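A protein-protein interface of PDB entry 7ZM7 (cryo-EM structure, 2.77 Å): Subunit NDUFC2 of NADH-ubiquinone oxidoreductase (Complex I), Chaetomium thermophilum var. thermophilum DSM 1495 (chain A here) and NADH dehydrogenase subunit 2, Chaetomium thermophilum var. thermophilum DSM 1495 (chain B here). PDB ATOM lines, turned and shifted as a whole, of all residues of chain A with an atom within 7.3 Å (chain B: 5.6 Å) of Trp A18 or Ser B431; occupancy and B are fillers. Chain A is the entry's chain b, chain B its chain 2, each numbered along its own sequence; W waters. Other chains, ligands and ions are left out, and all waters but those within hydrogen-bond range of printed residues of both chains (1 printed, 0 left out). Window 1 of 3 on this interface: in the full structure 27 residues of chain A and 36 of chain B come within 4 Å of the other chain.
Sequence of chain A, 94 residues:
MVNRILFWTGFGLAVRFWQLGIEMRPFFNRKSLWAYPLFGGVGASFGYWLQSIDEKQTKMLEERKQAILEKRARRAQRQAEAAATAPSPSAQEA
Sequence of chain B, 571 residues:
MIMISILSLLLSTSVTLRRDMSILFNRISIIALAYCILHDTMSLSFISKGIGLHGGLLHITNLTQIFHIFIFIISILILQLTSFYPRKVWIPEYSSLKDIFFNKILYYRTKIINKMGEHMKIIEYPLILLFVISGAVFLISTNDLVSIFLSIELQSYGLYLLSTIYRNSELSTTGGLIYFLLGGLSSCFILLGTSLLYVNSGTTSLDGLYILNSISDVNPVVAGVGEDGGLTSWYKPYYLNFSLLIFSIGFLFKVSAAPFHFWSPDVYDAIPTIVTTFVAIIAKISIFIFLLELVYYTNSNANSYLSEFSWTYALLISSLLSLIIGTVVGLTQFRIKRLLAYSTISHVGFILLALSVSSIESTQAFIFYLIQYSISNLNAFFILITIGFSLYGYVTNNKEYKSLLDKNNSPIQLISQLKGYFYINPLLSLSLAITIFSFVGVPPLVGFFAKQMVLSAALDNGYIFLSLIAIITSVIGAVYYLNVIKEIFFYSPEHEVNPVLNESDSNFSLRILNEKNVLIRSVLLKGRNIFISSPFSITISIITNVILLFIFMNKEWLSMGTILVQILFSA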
ATOM      1  N   GLY A  12      29.699  19.648  22.033  1.00  0.00           N
ATOM      2  CA  GLY A  12      30.773  19.300  21.086  1.00  0.00           C
ATOM      3  C   GLY A  12      30.443  18.036  20.313  1.00  0.00           C
ATOM      4  O   GLY A  12      30.680  18.013  19.106  1.00  0.00           O
ATOM      5  N   LEU A  13      29.877  17.028  20.970  1.00  0.00           N
ATOM      6  CA  LEU A  13      29.458  15.827  20.207  1.00  0.00           C
ATOM      7  C   LEU A  13      28.325  16.173  19.226  1.00  0.00           C
ATOM      8  O   LEU A  13      28.337  15.620  18.121  1.00  0.00           O
ATOM      9  CB  LEU A  13      29.080  14.702  21.172  1.00  0.00           C
ATOM     10  CG  LEU A  13      30.165  14.253  22.144  1.00  0.00           C
ATOM     11  CD1 LEU A  13      29.635  13.157  23.051  1.00  0.00           C
ATOM     12  CD2 LEU A  13      31.392  13.774  21.394  1.00  0.00           C
ATOM     13  N   ALA A  14      27.387  17.046  19.605  1.00  0.00           N
ATOM     14  CA  ALA A  14      26.309  17.496  18.691  1.00  0.00           C
ATOM     15  C   ALA A  14      26.888  18.260  17.502  1.00  0.00           C
ATOM     16  O   ALA A  14      26.367  18.088  16.396  1.00  0.00           O
ATOM     17  CB  ALA A  14      25.292  18.309  19.443  1.00  0.00           C
ATOM     18  N   VAL A  15      27.912  19.079  17.740  1.00  0.00           N
ATOM     19  CA  VAL A  15      28.541  19.880  16.653  1.00  0.00           C
ATOM     20  C   VAL A  15      29.190  18.952  15.618  1.00  0.00           C
ATOM     21  O   VAL A  15      29.052  19.236  14.424  1.00  0.00           O
ATOM     22  CB  VAL A  15      29.453  21.002  17.193  1.00  0.00           C
ATOM     23  CG1 VAL A  15      30.414  21.544  16.148  1.00  0.00           C
ATOM     24  CG2 VAL A  15      28.647  22.127  17.816  1.00  0.00           C
ATOM     25  N   ARG A  16      29.814  17.855  16.045  1.00  0.00           N
ATOM     26  CA  ARG A  16      30.370  16.890  15.062  1.00  0.00           C
ATOM     27  C   ARG A  16      29.240  16.265  14.228  1.00  0.00           C
ATOM     28  O   ARG A  16      29.425  16.150  13.000  1.00  0.00           O
ATOM     29  CB  ARG A  16      31.273  15.862  15.753  1.00  0.00           C
ATOM     30  CG  ARG A  16      32.016  14.940  14.802  1.00  0.00           C
ATOM     31  CD  ARG A  16      32.863  15.716  13.820  1.00  0.00           C
ATOM     32  NE  ARG A  16      33.488  14.824  12.865  1.00  0.00           N
ATOM     33  CZ  ARG A  16      34.469  15.174  12.051  1.00  0.00           C
ATOM     34  NH1 ARG A  16      34.982  14.288  11.217  1.00  0.00           N
ATOM     35  NH2 ARG A  16      34.953  16.399  12.092  1.00  0.00           N
ATOM     36  N   PHE A  17      28.121  15.886  14.852  1.00  0.00           N
ATOM     37  CA  PHE A  17      27.022  15.216  14.110  1.00  0.00           C
ATOM     38  C   PHE A  17      26.407  16.150  13.070  1.00  0.00           C
ATOM     39  O   PHE A  17      26.176  15.714  11.934  1.00  0.00           O
ATOM     40  CB  PHE A  17      25.935  14.703  15.048  1.00  0.00           C
ATOM     41  CG  PHE A  17      26.234  13.369  15.672  1.00  0.00           C
ATOM     42  CD1 PHE A  17      26.589  13.274  17.006  1.00  0.00           C
ATOM     43  CD2 PHE A  17      26.158  12.211  14.920  1.00  0.00           C
ATOM     44  CE1 PHE A  17      26.863  12.046  17.580  1.00  0.00           C
ATOM     45  CE2 PHE A  17      26.432  10.983  15.494  1.00  0.00           C
ATOM     46  CZ  PHE A  17      26.783  10.905  16.821  1.00  0.00           C
ATOM     47  N   TRP A  18      26.190  17.408  13.447  1.00  0.00           N
ATOM     48  CA  TRP A  18      25.629  18.412  12.513  1.00  0.00           C
ATOM     49  C   TRP A  18      26.593  18.667  11.356  1.00  0.00           C
ATOM     50  O   TRP A  18      26.113  18.772  10.239  1.00  0.00           O
ATOM     51  CB  TRP A  18      25.248  19.693  13.254  1.00  0.00           C
ATOM     52  CG  TRP A  18      23.833  19.720  13.736  1.00  0.00           C
ATOM     53  CD1 TRP A  18      23.346  19.208  14.903  1.00  0.00           C
ATOM     54  CD2 TRP A  18      22.711  20.297  13.048  1.00  0.00           C
ATOM     55  NE1 TRP A  18      21.996  19.423  14.984  1.00  0.00           N
ATOM     56  CE2 TRP A  18      21.579  20.084  13.860  1.00  0.00           C
ATOM     57  CE3 TRP A  18      22.553  20.965  11.831  1.00  0.00           C
ATOM     58  CZ2 TRP A  18      20.310  20.523  13.492  1.00  0.00           C
ATOM     59  CZ3 TRP A  18      21.296  21.391  11.468  1.00  0.00           C
ATOM     60  CH2 TRP A  18      20.193  21.175  12.288  1.00  0.00           C
ATOM     61  N   GLN A  19      27.900  18.740  11.615  1.00  0.00           N
ATOM     62  CA  GLN A  19      28.892  19.065  10.554  1.00  0.00           C
ATOM     63  C   GLN A  19      28.880  17.978   9.481  1.00  0.00           C
ATOM     64  O   GLN A  19      28.861  18.326   8.303  1.00  0.00           O
ATOM     65  CB  GLN A  19      30.285  19.154  11.166  1.00  0.00           C
ATOM     66  CG  GLN A  19      31.387  19.302  10.134  1.00  0.00           C
ATOM     67  CD  GLN A  19      32.629  18.532  10.496  1.00  0.00           C
ATOM     68  OE1 GLN A  19      33.031  18.477  11.653  1.00  0.00           O
ATOM     69  NE2 GLN A  19      33.250  17.933   9.495  1.00  0.00           N
ATOM     70  N   LEU A  20      28.850  16.709   9.885  1.00  0.00           N
ATOM     71  CA  LEU A  20      28.787  15.577   8.933  1.00  0.00           C
ATOM     72  C   LEU A  20      27.449  15.586   8.192  1.00  0.00           C
ATOM     73  O   LEU A  20      27.457  15.265   7.012  1.00  0.00           O
ATOM     74  CB  LEU A  20      29.046  14.294   9.723  1.00  0.00           C
ATOM     75  CG  LEU A  20      30.384  14.253  10.460  1.00  0.00           C
ATOM     76  CD1 LEU A  20      30.595  12.919  11.154  1.00  0.00           C
ATOM     77  CD2 LEU A  20      31.536  14.556   9.521  1.00  0.00           C
ATOM     78  N   GLY A  21      26.348  15.926   8.870  1.00  0.00           N
ATOM     79  CA  GLY A  21      25.017  16.044   8.240  1.00  0.00           C
ATOM     80  C   GLY A  21      24.980  17.154   7.207  1.00  0.00           C
ATOM     81  O   GLY A  21      24.329  16.953   6.185  1.00  0.00           O
ATOM     82  N   ILE A  22      25.680  18.262   7.448  1.00  0.00           N
ATOM     83  CA  ILE A  22      25.684  19.443   6.535  1.00  0.00           C
ATOM     84  C   ILE A  22      26.612  19.108   5.378  1.00  0.00           C
ATOM     85  O   ILE A  22      26.302  19.468   4.242  1.00  0.00           O
ATOM     86  CB  ILE A  22      26.133  20.700   7.303  1.00  0.00           C
ATOM     87  CG1 ILE A  22      25.060  21.177   8.283  1.00  0.00           C
ATOM     88  CG2 ILE A  22      26.556  21.812   6.355  1.00  0.00           C
ATOM     89  CD1 ILE A  22      25.587  22.108   9.338  1.00  0.00           C
ATOM     90  N   GLU A  23      27.704  18.413   5.673  1.00  0.00           N
ATOM     91  CA  GLU A  23      28.628  17.935   4.611  1.00  0.00           C
ATOM     92  C   GLU A  23      27.997  16.743   3.894  1.00  0.00           C
ATOM     93  O   GLU A  23      28.397  16.491   2.762  1.00  0.00           O
ATOM     94  CB  GLU A  23      29.992  17.620   5.217  1.00  0.00           C
ATOM     95  CG  GLU A  23      30.760  18.854   5.636  1.00  0.00           C
ATOM     96  CD  GLU A  23      32.203  18.576   6.012  1.00  0.00           C
ATOM     97  OE1 GLU A  23      32.952  19.539   6.234  1.00  0.00           O
ATOM     98  OE2 GLU A  23      32.574  17.394   6.076  1.00  0.00           O
ATOM     99  N   MET A  24      27.058  16.046   4.533  1.00  0.00           N
ATOM    100  CA  MET A  24      26.432  14.803   3.992  1.00  0.00           C
ATOM    101  C   MET A  24      27.467  13.670   3.988  1.00  0.00           C
ATOM    102  O   MET A  24      27.246  12.668   3.297  1.00  0.00           O
ATOM    103  CB  MET A  24      25.684  14.993   2.672  1.00  0.00           C
ATOM    104  CG  MET A  24      24.649  16.096   2.727  1.00  0.00           C
ATOM    105  SD  MET A  24      23.875  16.445   1.131  1.00  0.00           S
ATOM    106  CE  MET A  24      22.724  15.077   1.030  1.00  0.00           C
ATOM    107  N   PHE A  27      28.343   9.581   9.189  1.00  0.00           N
ATOM    108  CA  PHE A  27      28.663   9.639  10.629  1.00  0.00           C
ATOM    109  C   PHE A  27      29.307   8.300  10.969  1.00  0.00           C
ATOM    110  O   PHE A  27      28.989   7.310  10.277  1.00  0.00           O
ATOM    111  CB  PHE A  27      27.380   9.675  11.460  1.00  0.00           C
ATOM    112  CG  PHE A  27      26.312  10.673  11.105  1.00  0.00           C
ATOM    113  CD1 PHE A  27      26.593  12.022  10.995  1.00  0.00           C
ATOM    114  CD2 PHE A  27      24.997  10.262  10.956  1.00  0.00           C
ATOM    115  CE1 PHE A  27      25.592  12.929  10.689  1.00  0.00           C
ATOM    116  CE2 PHE A  27      23.997  11.170  10.653  1.00  0.00           C
ATOM    117  CZ  PHE A  27      24.297  12.505  10.524  1.00  0.00           C
ATOM    118  N   TYR A  36      35.099  12.696  17.415  1.00  0.00           N
ATOM    119  CA  TYR A  36      34.103  12.816  18.505  1.00  0.00           C
ATOM    120  C   TYR A  36      34.829  13.069  19.836  1.00  0.00           C
ATOM    121  O   TYR A  36      34.435  14.015  20.530  1.00  0.00           O
ATOM    122  CB  TYR A  36      33.171  11.602  18.519  1.00  0.00           C
ATOM    123  CG  TYR A  36      32.253  11.468  17.331  1.00  0.00           C
ATOM    124  CD1 TYR A  36      31.060  12.168  17.268  1.00  0.00           C
ATOM    125  CD2 TYR A  36      32.560  10.620  16.279  1.00  0.00           C
ATOM    126  CE1 TYR A  36      30.206  12.044  16.187  1.00  0.00           C
ATOM    127  CE2 TYR A  36      31.715  10.484  15.190  1.00  0.00           C
ATOM    128  CZ  TYR A  36      30.532  11.198  15.144  1.00  0.00           C
ATOM    129  OH  TYR A  36      29.692  11.070  14.076  1.00  0.00           O
ATOM    130  N   ASN B 379      25.121  33.579  10.597  1.00  0.00           N
ATOM    131  CA  ASN B 379      24.757  32.245  10.132  1.00  0.00           C
ATOM    132  C   ASN B 379      23.918  32.312   8.867  1.00  0.00           C
ATOM    133  O   ASN B 379      24.083  31.495   7.961  1.00  0.00           O
ATOM    134  CB  ASN B 379      24.012  31.488  11.230  1.00  0.00           C
ATOM    135  CG  ASN B 379      24.145  29.982  11.105  1.00  0.00           C
ATOM    136  OD1 ASN B 379      25.228  29.464  10.890  1.00  0.00           O
ATOM    137  ND2 ASN B 379      23.042  29.279  11.242  1.00  0.00           N
ATOM    138  N   ILE B 383      25.244  30.373   5.594  1.00  0.00           N
ATOM    139  CA  ILE B 383      24.440  29.343   4.945  1.00  0.00           C
ATOM    140  C   ILE B 383      24.235  29.691   3.485  1.00  0.00           C
ATOM    141  O   ILE B 383      24.382  28.841   2.606  1.00  0.00           O
ATOM    142  CB  ILE B 383      23.100  29.144   5.672  1.00  0.00           C
ATOM    143  CG1 ILE B 383      23.327  28.586   7.073  1.00  0.00           C
ATOM    144  CG2 ILE B 383      22.223  28.185   4.895  1.00  0.00           C
ATOM    145  CD1 ILE B 383      22.168  28.778   7.995  1.00  0.00           C
ATOM    146  N   PRO B 426      19.439  18.235   3.368  1.00  0.00           N
ATOM    147  CA  PRO B 426      18.452  18.427   4.424  1.00  0.00           C
ATOM    148  C   PRO B 426      18.872  19.184   5.694  1.00  0.00           C
ATOM    149  O   PRO B 426      18.145  20.035   6.114  1.00  0.00           O
ATOM    150  CB  PRO B 426      18.088  16.987   4.796  1.00  0.00           C
ATOM    151  CG  PRO B 426      18.486  16.159   3.604  1.00  0.00           C
ATOM    152  CD  PRO B 426      19.718  16.837   3.068  1.00  0.00           C
ATOM    153  N   LEU B 427      19.988  18.940   6.270  1.00  0.00           N
ATOM    154  CA  LEU B 427      20.443  19.650   7.496  1.00  0.00           C
ATOM    155  C   LEU B 427      20.875  21.087   7.196  1.00  0.00           C
ATOM    156  O   LEU B 427      20.692  21.914   8.084  1.00  0.00           O
ATOM    157  CB  LEU B 427      21.558  18.861   8.193  1.00  0.00           C
ATOM    158  CG  LEU B 427      21.126  17.945   9.333  1.00  0.00           C
ATOM    159  CD1 LEU B 427      20.652  16.608   8.791  1.00  0.00           C
ATOM    160  CD2 LEU B 427      22.275  17.736  10.302  1.00  0.00           C
ATOM    161  N   LEU B 428      21.482  21.362   6.002  1.00  0.00           N
ATOM    162  CA  LEU B 428      21.767  22.779   5.646  1.00  0.00           C
ATOM    163  C   LEU B 428      20.445  23.540   5.569  1.00  0.00           C
ATOM    164  O   LEU B 428      20.419  24.712   5.965  1.00  0.00           O
ATOM    165  CB  LEU B 428      22.536  22.851   4.329  1.00  0.00           C
ATOM    166  CG  LEU B 428      23.260  24.171   4.059  1.00  0.00           C
ATOM    167  CD1 LEU B 428      23.944  24.692   5.311  1.00  0.00           C
ATOM    168  CD2 LEU B 428      24.268  24.017   2.932  1.00  0.00           C
ATOM    169  N   SER B 429      19.392  22.888   5.098  1.00  0.00           N
ATOM    170  CA  SER B 429      18.043  23.493   5.019  1.00  0.00           C
ATOM    171  C   SER B 429      17.477  23.709   6.421  1.00  0.00           C
ATOM    172  O   SER B 429      16.813  24.724   6.605  1.00  0.00           O
ATOM    173  CB  SER B 429      17.173  22.626   4.214  1.00  0.00           C
ATOM    174  OG  SER B 429      17.760  22.394   2.948  1.00  0.00           O
ATOM    175  N   LEU B 430      17.749  22.902   7.378  1.00  0.00           N
ATOM    176  CA  LEU B 430      17.228  23.055   8.751  1.00  0.00           C
ATOM    177  C   LEU B 430      18.092  24.066   9.483  1.00  0.00           C
ATOM    178  O   LEU B 430      17.582  24.686  10.400  1.00  0.00           O
ATOM    179  CB  LEU B 430      17.258  21.684   9.423  1.00  0.00           C
ATOM    180  CG  LEU B 430      16.258  21.505  10.559  1.00  0.00           C
ATOM    181  CD1 LEU B 430      14.845  21.695  10.039  1.00  0.00           C
ATOM    182  CD2 LEU B 430      16.419  20.141  11.208  1.00  0.00           C
ATOM    183  N   SER B 431      19.397  24.175   9.113  1.00  0.00           N
ATOM    184  CA  SER B 431      20.171  25.274   9.661  1.00  0.00           C
ATOM    185  C   SER B 431      19.605  26.611   9.211  1.00  0.00           C
ATOM    186  O   SER B 431      19.533  27.556   9.998  1.00  0.00           O
ATOM    187  CB  SER B 431      21.622  25.126   9.243  1.00  0.00           C
ATOM    188  OG  SER B 431      22.085  23.856   9.612  1.00  0.00           O
ATOM    189  N   LEU B 432      19.211  26.712   7.943  1.00  0.00           N
ATOM    190  CA  LEU B 432      18.600  27.936   7.453  1.00  0.00           C
ATOM    191  C   LEU B 432      17.196  28.108   8.004  1.00  0.00           C
ATOM    192  O   LEU B 432      16.717  29.236   8.145  1.00  0.00           O
ATOM    193  CB  LEU B 432      18.576  27.936   5.930  1.00  0.00           C
ATOM    194  CG  LEU B 432      18.123  29.239   5.275  1.00  0.00           C
ATOM    195  CD1 LEU B 432      18.893  30.425   5.841  1.00  0.00           C
ATOM    196  CD2 LEU B 432      18.261  29.164   3.786  1.00  0.00           C
ATOM    197  N   ALA B 433      16.545  27.014   8.375  1.00  0.00           N
ATOM    198  CA  ALA B 433      15.215  27.089   9.013  1.00  0.00           C
ATOM    199  C   ALA B 433      15.392  27.585  10.445  1.00  0.00           C
ATOM    200  O   ALA B 433      14.754  28.581  10.779  1.00  0.00           O
ATOM    201  CB  ALA B 433      14.561  25.732   8.975  1.00  0.00           C
ATOM    202  N   ILE B 434      16.291  26.967  11.216  1.00  0.00           N
ATOM    203  CA  ILE B 434      16.501  27.318  12.650  1.00  0.00           C
ATOM    204  C   ILE B 434      16.915  28.785  12.750  1.00  0.00           C
ATOM    205  O   ILE B 434      16.439  29.465  13.648  1.00  0.00           O
ATOM    206  CB  ILE B 434      17.521  26.352  13.286  1.00  0.00           C
ATOM    207  CG1 ILE B 434      16.897  24.980  13.546  1.00  0.00           C
ATOM    208  CG2 ILE B 434      18.129  26.932  14.553  1.00  0.00           C
ATOM    209  CD1 ILE B 434      17.865  23.834  13.464  1.00  0.00           C
ATOM    210  N   THR B 435      17.669  29.274  11.775  1.00  0.00           N
ATOM    211  CA  THR B 435      18.164  30.665  11.798  1.00  0.00           C
ATOM    212  C   THR B 435      17.024  31.616  11.438  1.00  0.00           C
ATOM    213  O   THR B 435      16.899  32.646  12.096  1.00  0.00           O
ATOM    214  CB  THR B 435      19.281  30.806  10.766  1.00  0.00           C
ATOM    215  OG1 THR B 435      20.256  29.826  11.115  1.00  0.00           O
ATOM    216  CG2 THR B 435      19.910  32.181  10.748  1.00  0.00           C
ATOM    217  N   ILE B 436      16.190  31.243  10.476  1.00  0.00           N
ATOM    218  CA  ILE B 436      15.114  32.132  10.065  1.00  0.00           C
ATOM    219  C   ILE B 436      14.008  32.169  11.112  1.00  0.00           C
ATOM    220  O   ILE B 436      13.433  33.223  11.393  1.00  0.00           O
ATOM    221  CB  ILE B 436      14.607  31.693   8.680  1.00  0.00           C
ATOM    222  CG1 ILE B 436      15.539  32.229   7.603  1.00  0.00           C
ATOM    223  CG2 ILE B 436      13.196  32.134   8.435  1.00  0.00           C
ATOM    224  CD1 ILE B 436      15.173  31.827   6.257  1.00  0.00           C
ATOM    225  N   ILE B 540      28.849  26.812  10.804  1.00  0.00           N
ATOM    226  CA  ILE B 540      27.395  26.787  10.704  1.00  0.00           C
ATOM    227  C   ILE B 540      26.795  25.970  11.834  1.00  0.00           C
ATOM    228  O   ILE B 540      25.801  26.369  12.448  1.00  0.00           O
ATOM    229  CB  ILE B 540      26.969  26.241   9.333  1.00  0.00           C
ATOM    230  CG1 ILE B 540      27.187  27.291   8.247  1.00  0.00           C
ATOM    231  CG2 ILE B 540      25.528  25.766   9.362  1.00  0.00           C
ATOM    232  CD1 ILE B 540      27.197  26.720   6.854  1.00  0.00           C
ATOM    233  N   SER B 541      27.401  24.826  12.147  1.00  0.00           N
ATOM    234  CA  SER B 541      26.825  23.953  13.156  1.00  0.00           C
ATOM    235  C   SER B 541      26.991  24.508  14.566  1.00  0.00           C
ATOM    236  O   SER B 541      26.221  24.149  15.457  1.00  0.00           O
ATOM    237  CB  SER B 541      27.416  22.548  13.037  1.00  0.00           C
ATOM    238  OG  SER B 541      28.763  22.495  13.418  1.00  0.00           O
ATOM    239  N   THR B 544      24.104  27.310  14.715  1.00  0.00           N
ATOM    240  CA  THR B 544      22.747  26.729  14.668  1.00  0.00           C
ATOM    241  C   THR B 544      22.474  26.091  16.036  1.00  0.00           C
ATOM    242  O   THR B 544      21.354  26.251  16.529  1.00  0.00           O
ATOM    243  CB  THR B 544      22.591  25.899  13.384  1.00  0.00           C
ATOM    244  OG1 THR B 544      22.326  26.804  12.315  1.00  0.00           O
ATOM    245  CG2 THR B 544      21.497  24.856  13.463  1.00  0.00           C
ATOM    246  N   ASN B 545      23.462  25.403  16.607  1.00  0.00           N
ATOM    247  CA  ASN B 545      23.344  24.762  17.944  1.00  0.00           C
ATOM    248  C   ASN B 545      23.174  25.791  19.066  1.00  0.00           C
ATOM    249  O   ASN B 545      22.401  25.527  19.972  1.00  0.00           O
ATOM    250  CB  ASN B 545      24.487  23.785  18.203  1.00  0.00           C
ATOM    251  CG  ASN B 545      24.329  22.477  17.460  1.00  0.00           C
ATOM    252  OD1 ASN B 545      23.658  22.410  16.433  1.00  0.00           O
ATOM    253  ND2 ASN B 545      24.959  21.432  17.964  1.00  0.00           N
ATOM    254  N   LEU B 548      19.612  26.918  18.866  1.00  0.00           N
ATOM    255  CA  LEU B 548      18.672  25.847  19.269  1.00  0.00           C
ATOM    256  C   LEU B 548      18.841  25.447  20.739  1.00  0.00           C
ATOM    257  O   LEU B 548      17.834  25.041  21.333  1.00  0.00           O
ATOM    258  CB  LEU B 548      18.874  24.661  18.321  1.00  0.00           C
ATOM    259  CG  LEU B 548      17.885  23.510  18.475  1.00  0.00           C
ATOM    260  CD1 LEU B 548      16.748  23.637  17.473  1.00  0.00           C
ATOM    261  CD2 LEU B 548      18.586  22.170  18.328  1.00  0.00           C
HETATM  262  O   HOH W   1      22.006  17.191   5.131  1.00  0.00           O
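The backbone carbonyl oxygen (O) of Val A15 sits close to the side-chain hydroxyl (OG) of Ser B541.
The side-chain hydroxyl (OG) of Ser B431 lies within hydrogen-bond range of the backbone carbonyl oxygen (O) of Leu B427, at 2.8 Å. The backbone carbonyl oxygen (O) of Ser B431 lies within hydrogen-bond range of the side-chain hydroxyl (OG1) of Thr B435 (2.6 Å). The backbone carbonyl oxygen (O) of Ser B541 lies close to the side-chain amide oxygen (OD1) of Asn B545, at 3.2 Å.
Among the printed residues, pairs that only touch across the chains: Trp A18 with Ser B431 (3.2 Å), Ala A14 with Asn B545 (3.5 Å), Trp A18 with Leu B427 (3.5 Å), Trp A18 with Asn B545 (3.6 Å), Trp A18 with Ser B541 (3.6 Å), Ile A22 with Ile B540 (3.7 Å), Trp A18 with Ile B434 (3.7 Å), Val A15 with Asn B545 (3.8 Å), Gly A21 with Leu B427 (3.8 Å) and Ile A22 with Ser B431 (3.9 Å).
Printed residues of chain B within 4 Å of Val A15: Ser B541 and Asn B545. Of the printed residues of chain B, Trp A18 touches Leu B427 (3.5 Å), Ser B431 (3.2 Å), Ile B434 (3.7 Å), Ser B541 (3.6 Å) and Asn B545 (3.6 Å). Ser B431 touches just these residues of chain A: Trp A18 and Ile A22. Of the printed residues of chain A, Ile B540 touches Ile A22 (3.7 Å). Of the printed residues of chain A, Ser B541 touches Val A15 (3.3 Å) and Trp A18 (3.6 Å). Printed residues of chain A within 4 Å of Asn B545: Ala A14, Val A15 and Trp A18.
Printed residues of chain B that touch a printed residue of chain A: Leu B427, Ser B431, Ile B434, Ile B540, Ser B541 and Asn B545. Hydrophobic or aromatic side chains of chain B within 4 Å of the printed part of chain A: Leu B427, Ile B434 and Ile B540. Along chain B the printed residues that touch a printed residue of chain A span positions 427 to 545. Among the printed residues, no Asp or Glu carboxylate lies within 4 Å of a Lys or Arg side-chain nitrogen of the other chain.
Water W1 bridges O of Gly A21 and N of Leu B427.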
